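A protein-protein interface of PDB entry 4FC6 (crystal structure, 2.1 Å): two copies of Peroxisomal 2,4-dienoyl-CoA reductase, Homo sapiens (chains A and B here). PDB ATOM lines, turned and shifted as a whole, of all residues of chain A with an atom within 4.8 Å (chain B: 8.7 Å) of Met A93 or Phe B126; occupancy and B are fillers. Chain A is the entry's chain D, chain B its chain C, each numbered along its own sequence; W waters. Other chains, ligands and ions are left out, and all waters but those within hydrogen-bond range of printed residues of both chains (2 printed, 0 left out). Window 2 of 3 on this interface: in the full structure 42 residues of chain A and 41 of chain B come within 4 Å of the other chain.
The backbone carbonyl oxygen of Leu B124 sits at hydrogen-bond distance from the guanidinium group of Arg A145 (2.9 Å). The guanidinium group of Arg A145 sits close to the backbone carbonyl oxygen of Gly B122.
CG of Phe B126 touches CG of Pro A89 (3.6 Å). Phe B126 touches Met A93. Phe A141 touches Ala B121. CZ of Phe A141 touches O of Leu B124, 3.7 Å away. Phe B129 touches Phe A141 (CB to CE2, 3.6 Å). Asn A142 touches Phe B126. Ala B121 touches Arg A145. C of Ala B123 touches NH2 of Arg A145, at 3.8 Å. CG of Arg A145 touches CE1 of Phe B126, at 3.6 Å. Val A146 touches Phe B126.
Of the printed residues of chain B, Met A93 touches Phe B126 (3.4 Å). Of chain A, only Pro A89, Met A93, Asn A142, Arg A145 and Val A146 come within 4 Å of Phe B126. Of the printed residues of chain B, Pro A89 touches Phe B126 (3.6 Å). Of the printed residues of chain A, Leu B124 touches Phe A141 (3.7 Å) and Arg A145 (2.9 Å). Of the printed residues of chain A, Ala B121 touches Phe A141 and Arg A145. Printed residues of chain B within 4 Å of Val A146: Phe B126 (3.6 Å). Ala A91 touches none of the printed residues of chain B. Ser B125 touches none of the printed residues of chain A. The nearest residue of chain B that does not touch Met A93 is Ser B125 (8.6 Å). The nearest residue of chain A that does not touch Phe B126 is Phe A141 (4.2 Å). The nearest printed residue of chain A that does not touch Gly B122 is Phe A141 (6.0 Å).
Of the 15 printed residues of chain B, 6 touch a printed residue of chain A. Printed residues of chain B that touch a printed residue of chain A: Ala B121, Gly B122, Ala B123, Leu B124, Phe B126 and Phe B129. Hydrophobic or aromatic side chains of chain B within 4 Å of the printed part of chain A: Leu B124, Phe B126 and Phe B129. Of the 14 printed residues of chain A, 6 touch a printed residue of chain B. Hydrophobic or aromatic side chains of chain A that line the printed part of chain B: Pro A89, Met A93, Phe A141 and Val A146. Among the printed residues, no Asp or Glu carboxylate lies within 4 Å of a Lys or Arg side-chain nitrogen of the other chain.
No position is printed for both chains. Of the 12 pairs that touch across the chains among the printed residues, none has its exchanged pair printed and touching as well.
Water W2 lies within hydrogen-bond range of the backbone carbonyl oxygen (O) of Phe B126 (2.7 Å) and the side-chain amide oxygen (OD1) of Asn A142 (2.9 Å). Water W1 bridges O of Ala B123 (2.9 Å) and NH2 of Arg A145 (3.2 Å).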
ATOM      1  N   PRO A  89      16.442 -18.431  -4.679  1.00  0.00           N
ATOM      2  CA  PRO A  89      16.498 -19.292  -5.875  1.00  0.00           C
ATOM      3  C   PRO A  89      17.845 -19.237  -6.708  1.00  0.00           C
ATOM      4  O   PRO A  89      18.292 -20.271  -7.222  1.00  0.00           O
ATOM      5  CB  PRO A  89      15.306 -18.823  -6.696  1.00  0.00           C
ATOM      6  CG  PRO A  89      14.347 -18.224  -5.652  1.00  0.00           C
ATOM      7  CD  PRO A  89      15.272 -17.536  -4.678  1.00  0.00           C
ATOM      8  N   PRO A  90      18.486 -18.054  -6.813  1.00  0.00           N
ATOM      9  CA  PRO A  90      19.729 -18.034  -7.601  1.00  0.00           C
ATOM     10  C   PRO A  90      20.827 -18.845  -6.910  1.00  0.00           C
ATOM     11  O   PRO A  90      21.585 -19.511  -7.602  1.00  0.00           O
ATOM     12  CB  PRO A  90      20.098 -16.534  -7.653  1.00  0.00           C
ATOM     13  CG  PRO A  90      18.770 -15.792  -7.384  1.00  0.00           C
ATOM     14  CD  PRO A  90      18.074 -16.697  -6.386  1.00  0.00           C
ATOM     15  N   ALA A  91      20.874 -18.818  -5.572  1.00  0.00           N
ATOM     16  CA  ALA A  91      21.836 -19.658  -4.814  1.00  0.00           C
ATOM     17  C   ALA A  91      21.538 -21.154  -4.915  1.00  0.00           C
ATOM     18  O   ALA A  91      22.466 -22.028  -5.010  1.00  0.00           O
ATOM     19  CB  ALA A  91      21.920 -19.207  -3.354  1.00  0.00           C
ATOM     20  N   VAL A  92      20.243 -21.485  -4.953  1.00  0.00           N
ATOM     21  CA  VAL A  92      19.847 -22.873  -5.129  1.00  0.00           C
ATOM     22  C   VAL A  92      20.275 -23.367  -6.481  1.00  0.00           C
ATOM     23  O   VAL A  92      20.868 -24.437  -6.604  1.00  0.00           O
ATOM     24  CB  VAL A  92      18.323 -23.058  -4.890  1.00  0.00           C
ATOM     25  CG1 VAL A  92      17.889 -24.509  -5.145  1.00  0.00           C
ATOM     26  CG2 VAL A  92      18.019 -22.664  -3.432  1.00  0.00           C
ATOM     27  N   MET A  93      19.977 -22.566  -7.503  1.00  0.00           N
ATOM     28  CA  MET A  93      20.431 -22.840  -8.859  1.00  0.00           C
ATOM     29  C   MET A  93      21.949 -23.024  -8.956  1.00  0.00           C
ATOM     30  O   MET A  93      22.401 -24.049  -9.476  1.00  0.00           O
ATOM     31  CB  MET A  93      19.989 -21.719  -9.804  1.00  0.00           C
ATOM     32  CG  MET A  93      18.499 -21.769 -10.188  1.00  0.00           C
ATOM     33  SD  MET A  93      18.056 -20.189 -10.966  1.00  0.00           S
ATOM     34  CE  MET A  93      16.537 -19.901 -10.078  1.00  0.00           C
ATOM     35  N   ALA A  94      22.706 -22.032  -8.484  1.00  0.00           N
ATOM     36  CA  ALA A  94      24.172 -22.175  -8.398  1.00  0.00           C
ATOM     37  C   ALA A  94      24.597 -23.490  -7.688  1.00  0.00           C
ATOM     38  O   ALA A  94      25.405 -24.222  -8.254  1.00  0.00           O
ATOM     39  CB  ALA A  94      24.795 -20.978  -7.721  1.00  0.00           C
ATOM     40  N   ALA A  95      24.028 -23.814  -6.508  1.00  0.00           N
ATOM     41  CA  ALA A  95      24.336 -25.126  -5.832  1.00  0.00           C
ATOM     42  C   ALA A  95      24.032 -26.369  -6.694  1.00  0.00           C
ATOM     43  O   ALA A  95      24.868 -27.276  -6.817  1.00  0.00           O
ATOM     44  CB  ALA A  95      23.645 -25.245  -4.495  1.00  0.00           C
ATOM     45  N   VAL A  96      22.858 -26.427  -7.294  1.00  0.00           N
ATOM     46  CA  VAL A  96      22.499 -27.586  -8.119  1.00  0.00           C
ATOM     47  C   VAL A  96      23.410 -27.652  -9.387  1.00  0.00           C
ATOM     48  O   VAL A  96      23.801 -28.751  -9.842  1.00  0.00           O
ATOM     49  CB  VAL A  96      20.992 -27.513  -8.464  1.00  0.00           C
ATOM     50  CG1 VAL A  96      20.557 -28.585  -9.477  1.00  0.00           C
ATOM     51  CG2 VAL A  96      20.138 -27.573  -7.184  1.00  0.00           C
ATOM     52  N   ASP A  97      23.779 -26.486  -9.940  1.00  0.00           N
ATOM     53  CA  ASP A  97      24.678 -26.492 -11.079  1.00  0.00           C
ATOM     54  C   ASP A  97      26.014 -27.124 -10.679  1.00  0.00           C
ATOM     55  O   ASP A  97      26.529 -28.024 -11.377  1.00  0.00           O
ATOM     56  CB  ASP A  97      24.905 -25.075 -11.606  1.00  0.00           C
ATOM     57  CG  ASP A  97      23.762 -24.600 -12.451  1.00  0.00           C
ATOM     58  OD1 ASP A  97      22.945 -25.439 -12.886  1.00  0.00           O
ATOM     59  OD2 ASP A  97      23.653 -23.382 -12.669  1.00  0.00           O
ATOM     60  N   PHE A 141       9.667 -25.896  -1.840  1.00  0.00           N
ATOM     61  CA  PHE A 141       9.219 -25.733  -3.196  1.00  0.00           C
ATOM     62  C   PHE A 141      10.403 -25.309  -4.096  1.00  0.00           C
ATOM     63  O   PHE A 141      10.617 -25.869  -5.168  1.00  0.00           O
ATOM     64  CB  PHE A 141       8.019 -24.772  -3.341  1.00  0.00           C
ATOM     65  CG  PHE A 141       7.700 -24.453  -4.781  1.00  0.00           C
ATOM     66  CD1 PHE A 141       6.994 -25.391  -5.589  1.00  0.00           C
ATOM     67  CD2 PHE A 141       8.199 -23.303  -5.382  1.00  0.00           C
ATOM     68  CE1 PHE A 141       6.757 -25.132  -6.946  1.00  0.00           C
ATOM     69  CE2 PHE A 141       7.947 -23.034  -6.739  1.00  0.00           C
ATOM     70  CZ  PHE A 141       7.223 -23.958  -7.512  1.00  0.00           C
ATOM     71  N   ASN A 142      11.109 -24.279  -3.669  1.00  0.00           N
ATOM     72  CA  ASN A 142      12.266 -23.735  -4.396  1.00  0.00           C
ATOM     73  C   ASN A 142      13.265 -24.802  -4.815  1.00  0.00           C
ATOM     74  O   ASN A 142      13.583 -24.874  -6.010  1.00  0.00           O
ATOM     75  CB  ASN A 142      12.945 -22.628  -3.580  1.00  0.00           C
ATOM     76  CG  ASN A 142      12.113 -21.342  -3.565  1.00  0.00           C
ATOM     77  OD1 ASN A 142      11.162 -21.212  -4.355  1.00  0.00           O
ATOM     78  ND2 ASN A 142      12.486 -20.385  -2.725  1.00  0.00           N
ATOM     79  N   ARG A 145      11.623 -27.368  -7.128  1.00  0.00           N
ATOM     80  CA  ARG A 145      11.399 -26.693  -8.415  1.00  0.00           C
ATOM     81  C   ARG A 145      12.706 -26.574  -9.224  1.00  0.00           C
ATOM     82  O   ARG A 145      12.712 -26.859 -10.462  1.00  0.00           O
ATOM     83  CB  ARG A 145      10.767 -25.326  -8.178  1.00  0.00           C
ATOM     84  CG  ARG A 145      10.584 -24.432  -9.406  1.00  0.00           C
ATOM     85  CD  ARG A 145       9.763 -25.071 -10.499  1.00  0.00           C
ATOM     86  NE  ARG A 145       9.466 -24.058 -11.511  1.00  0.00           N
ATOM     87  CZ  ARG A 145      10.285 -23.740 -12.514  1.00  0.00           C
ATOM     88  NH1 ARG A 145      11.458 -24.381 -12.674  1.00  0.00           N
ATOM     89  NH2 ARG A 145       9.923 -22.795 -13.360  1.00  0.00           N
ATOM     90  N   VAL A 146      13.812 -26.251  -8.554  1.00  0.00           N
ATOM     91  CA  VAL A 146      15.113 -26.155  -9.273  1.00  0.00           C
ATOM     92  C   VAL A 146      15.640 -27.536  -9.716  1.00  0.00           C
ATOM     93  O   VAL A 146      16.090 -27.697 -10.848  1.00  0.00           O
ATOM     94  CB  VAL A 146      16.178 -25.411  -8.492  1.00  0.00           C
ATOM     95  CG1 VAL A 146      17.531 -25.517  -9.238  1.00  0.00           C
ATOM     96  CG2 VAL A 146      15.755 -23.942  -8.300  1.00  0.00           C
ATOM     97  N   LYS A 150      16.513 -28.596 -13.574  1.00  0.00           N
ATOM     98  CA  LYS A 150      17.902 -28.840 -13.868  1.00  0.00           C
ATOM     99  C   LYS A 150      18.233 -30.336 -14.132  1.00  0.00           C
ATOM    100  O   LYS A 150      19.248 -30.616 -14.759  1.00  0.00           O
ATOM    101  CB  LYS A 150      18.788 -28.232 -12.751  1.00  0.00           C
ATOM    102  CG  LYS A 150      18.741 -26.703 -12.790  1.00  0.00           C
ATOM    103  CD  LYS A 150      19.995 -26.069 -12.180  1.00  0.00           C
ATOM    104  CE  LYS A 150      20.071 -24.542 -12.391  1.00  0.00           C
ATOM    105  NZ  LYS A 150      20.645 -24.122 -13.700  1.00  0.00           N
ATOM    106  N   ALA B 121       3.209 -26.994 -11.687  1.00  0.00           N
ATOM    107  CA  ALA B 121       4.250 -26.812 -10.684  1.00  0.00           C
ATOM    108  C   ALA B 121       5.643 -26.642 -11.335  1.00  0.00           C
ATOM    109  O   ALA B 121       6.463 -25.850 -10.868  1.00  0.00           O
ATOM    110  CB  ALA B 121       4.233 -28.014  -9.727  1.00  0.00           C
ATOM    111  N   GLY B 122       5.901 -27.355 -12.435  1.00  0.00           N
ATOM    112  CA  GLY B 122       7.150 -27.173 -13.197  1.00  0.00           C
ATOM    113  C   GLY B 122       7.334 -25.843 -13.933  1.00  0.00           C
ATOM    114  O   GLY B 122       8.463 -25.452 -14.181  1.00  0.00           O
ATOM    115  N   ALA B 123       6.247 -25.134 -14.283  1.00  0.00           N
ATOM    116  CA  ALA B 123       6.338 -23.763 -14.825  1.00  0.00           C
ATOM    117  C   ALA B 123       6.133 -22.676 -13.757  1.00  0.00           C
ATOM    118  O   ALA B 123       6.314 -21.500 -14.063  1.00  0.00           O
ATOM    119  CB  ALA B 123       5.318 -23.530 -15.974  1.00  0.00           C
ATOM    120  N   LEU B 124       5.722 -23.028 -12.528  1.00  0.00           N
ATOM    121  CA  LEU B 124       5.420 -21.983 -11.542  1.00  0.00           C
ATOM    122  C   LEU B 124       6.718 -21.332 -11.071  1.00  0.00           C
ATOM    123  O   LEU B 124       7.611 -22.049 -10.608  1.00  0.00           O
ATOM    124  CB  LEU B 124       4.703 -22.595 -10.326  1.00  0.00           C
ATOM    125  CG  LEU B 124       4.168 -21.710  -9.199  1.00  0.00           C
ATOM    126  CD1 LEU B 124       3.066 -20.837  -9.768  1.00  0.00           C
ATOM    127  CD2 LEU B 124       3.596 -22.596  -8.059  1.00  0.00           C
ATOM    128  N   SER B 125       6.831 -20.002 -11.115  1.00  0.00           N
ATOM    129  CA  SER B 125       8.017 -19.340 -10.530  1.00  0.00           C
ATOM    130  C   SER B 125       8.009 -19.385  -9.025  1.00  0.00           C
ATOM    131  O   SER B 125       6.964 -19.523  -8.395  1.00  0.00           O
ATOM    132  CB  SER B 125       8.154 -17.871 -10.960  1.00  0.00           C
ATOM    133  OG  SER B 125       7.293 -17.088 -10.185  1.00  0.00           O
ATOM    134  N   PHE B 126       9.191 -19.222  -8.447  1.00  0.00           N
ATOM    135  CA  PHE B 126       9.383 -19.128  -6.994  1.00  0.00           C
ATOM    136  C   PHE B 126       8.545 -17.977  -6.401  1.00  0.00           C
ATOM    137  O   PHE B 126       7.922 -18.114  -5.333  1.00  0.00           O
ATOM    138  CB  PHE B 126      10.864 -18.915  -6.743  1.00  0.00           C
ATOM    139  CG  PHE B 126      11.767 -19.776  -7.662  1.00  0.00           C
ATOM    140  CD1 PHE B 126      11.995 -21.142  -7.387  1.00  0.00           C
ATOM    141  CD2 PHE B 126      12.376 -19.232  -8.792  1.00  0.00           C
ATOM    142  CE1 PHE B 126      12.823 -21.915  -8.198  1.00  0.00           C
ATOM    143  CE2 PHE B 126      13.205 -20.014  -9.618  1.00  0.00           C
ATOM    144  CZ  PHE B 126      13.424 -21.356  -9.325  1.00  0.00           C
ATOM    145  N   ASN B 127       8.532 -16.845  -7.098  1.00  0.00           N
ATOM    146  CA  ASN B 127       7.766 -15.683  -6.660  1.00  0.00           C
ATOM    147  C   ASN B 127       6.288 -16.035  -6.731  1.00  0.00           C
ATOM    148  O   ASN B 127       5.556 -15.656  -5.867  1.00  0.00           O
ATOM    149  CB  ASN B 127       8.071 -14.405  -7.512  1.00  0.00           C
ATOM    150  CG  ASN B 127       7.440 -13.106  -6.929  1.00  0.00           C
ATOM    151  OD1 ASN B 127       7.387 -12.945  -5.680  1.00  0.00           O
ATOM    152  ND2 ASN B 127       7.007 -12.130  -7.831  1.00  0.00           N
ATOM    153  N   ALA B 128       5.859 -16.741  -7.777  1.00  0.00           N
ATOM    154  CA  ALA B 128       4.443 -17.042  -7.886  1.00  0.00           C
ATOM    155  C   ALA B 128       3.970 -17.922  -6.723  1.00  0.00           C
ATOM    156  O   ALA B 128       2.943 -17.653  -6.150  1.00  0.00           O
ATOM    157  CB  ALA B 128       4.106 -17.692  -9.189  1.00  0.00           C
ATOM    158  N   PHE B 129       4.707 -18.993  -6.430  1.00  0.00           N
ATOM    159  CA  PHE B 129       4.408 -19.869  -5.309  1.00  0.00           C
ATOM    160  C   PHE B 129       4.350 -19.073  -4.033  1.00  0.00           C
ATOM    161  O   PHE B 129       3.409 -19.206  -3.261  1.00  0.00           O
ATOM    162  CB  PHE B 129       5.437 -20.987  -5.161  1.00  0.00           C
ATOM    163  CG  PHE B 129       5.119 -21.929  -4.038  1.00  0.00           C
ATOM    164  CD1 PHE B 129       4.269 -23.008  -4.244  1.00  0.00           C
ATOM    165  CD2 PHE B 129       5.603 -21.700  -2.753  1.00  0.00           C
ATOM    166  CE1 PHE B 129       3.957 -23.891  -3.199  1.00  0.00           C
ATOM    167  CE2 PHE B 129       5.262 -22.560  -1.728  1.00  0.00           C
ATOM    168  CZ  PHE B 129       4.451 -23.669  -1.975  1.00  0.00           C
ATOM    169  N   LYS B 130       5.361 -18.260  -3.790  1.00  0.00           N
ATOM    170  CA  LYS B 130       5.453 -17.550  -2.494  1.00  0.00           C
ATOM    171  C   LYS B 130       4.371 -16.484  -2.344  1.00  0.00           C
ATOM    172  O   LYS B 130       3.909 -16.243  -1.229  1.00  0.00           O
ATOM    173  CB  LYS B 130       6.824 -16.893  -2.329  1.00  0.00           C
ATOM    174  CG  LYS B 130       7.105 -16.490  -0.913  1.00  0.00           C
ATOM    175  CD  LYS B 130       8.575 -16.180  -0.718  1.00  0.00           C
ATOM    176  CE  LYS B 130       8.702 -14.867   0.010  1.00  0.00           C
ATOM    177  NZ  LYS B 130       7.656 -14.756   1.102  1.00  0.00           N
ATOM    178  N   THR B 131       3.955 -15.850  -3.462  1.00  0.00           N
ATOM    179  CA  THR B 131       2.949 -14.834  -3.360  1.00  0.00           C
ATOM    180  C   THR B 131       1.623 -15.410  -2.823  1.00  0.00           C
ATOM    181  O   THR B 131       0.933 -14.769  -2.055  1.00  0.00           O
ATOM    182  CB  THR B 131       2.713 -14.162  -4.735  1.00  0.00           C
ATOM    183  OG1 THR B 131       3.913 -13.485  -5.153  1.00  0.00           O
ATOM    184  CG2 THR B 131       1.540 -13.166  -4.654  1.00  0.00           C
ATOM    185  N   VAL B 132       1.258 -16.602  -3.296  1.00  0.00           N
ATOM    186  CA  VAL B 132       0.024 -17.275  -2.866  1.00  0.00           C
ATOM    187  C   VAL B 132       0.104 -17.645  -1.394  1.00  0.00           C
ATOM    188  O   VAL B 132      -0.865 -17.429  -0.659  1.00  0.00           O
ATOM    189  CB  VAL B 132      -0.368 -18.470  -3.792  1.00  0.00           C
ATOM    190  CG1 VAL B 132      -1.549 -19.265  -3.218  1.00  0.00           C
ATOM    191  CG2 VAL B 132      -0.746 -17.914  -5.188  1.00  0.00           C
ATOM    192  N   MET B 133       1.282 -18.112  -0.969  1.00  0.00           N
ATOM    193  CA  MET B 133       1.563 -18.462   0.430  1.00  0.00           C
ATOM    194  C   MET B 133       1.338 -17.229   1.285  1.00  0.00           C
ATOM    195  O   MET B 133       0.819 -17.302   2.379  1.00  0.00           O
ATOM    196  CB  MET B 133       3.039 -18.813   0.644  1.00  0.00           C
ATOM    197  CG  MET B 133       3.491 -20.186   0.222  1.00  0.00           C
ATOM    198  SD  MET B 133       2.408 -21.466   0.847  1.00  0.00           S
ATOM    199  CE  MET B 133       1.436 -21.563  -0.639  1.00  0.00           C
ATOM    200  N   ASP B 134       1.821 -16.092   0.771  1.00  0.00           N
ATOM    201  CA  ASP B 134       1.837 -14.860   1.510  1.00  0.00           C
ATOM    202  C   ASP B 134       0.407 -14.340   1.756  1.00  0.00           C
ATOM    203  O   ASP B 134       0.112 -13.897   2.846  1.00  0.00           O
ATOM    204  CB  ASP B 134       2.669 -13.786   0.774  1.00  0.00           C
ATOM    205  CG  ASP B 134       4.184 -13.983   0.922  1.00  0.00           C
ATOM    206  OD1 ASP B 134       4.646 -14.760   1.818  1.00  0.00           O
ATOM    207  OD2 ASP B 134       4.913 -13.348   0.113  1.00  0.00           O
ATOM    208  N   HIS B 176       0.513 -24.374  -5.234  1.00  0.00           N
ATOM    209  CA  HIS B 176       0.526 -23.121  -4.460  1.00  0.00           C
ATOM    210  C   HIS B 176      -0.727 -22.979  -3.616  1.00  0.00           C
ATOM    211  O   HIS B 176      -0.653 -22.828  -2.392  1.00  0.00           O
ATOM    212  CB  HIS B 176       0.719 -21.894  -5.404  1.00  0.00           C
ATOM    213  CG  HIS B 176      -0.122 -21.973  -6.695  1.00  0.00           C
ATOM    214  ND1 HIS B 176       0.154 -22.857  -7.684  1.00  0.00           N
ATOM    215  CD2 HIS B 176      -1.268 -21.277  -7.099  1.00  0.00           C
ATOM    216  CE1 HIS B 176      -0.773 -22.737  -8.682  1.00  0.00           C
ATOM    217  NE2 HIS B 176      -1.632 -21.754  -8.328  1.00  0.00           N
HETATM  218  O   HOH W   1       8.767 -19.916 -14.062  1.00  0.00           O
HETATM  219  O   HOH W   2       8.896 -19.688  -3.391  1.00  0.00           O
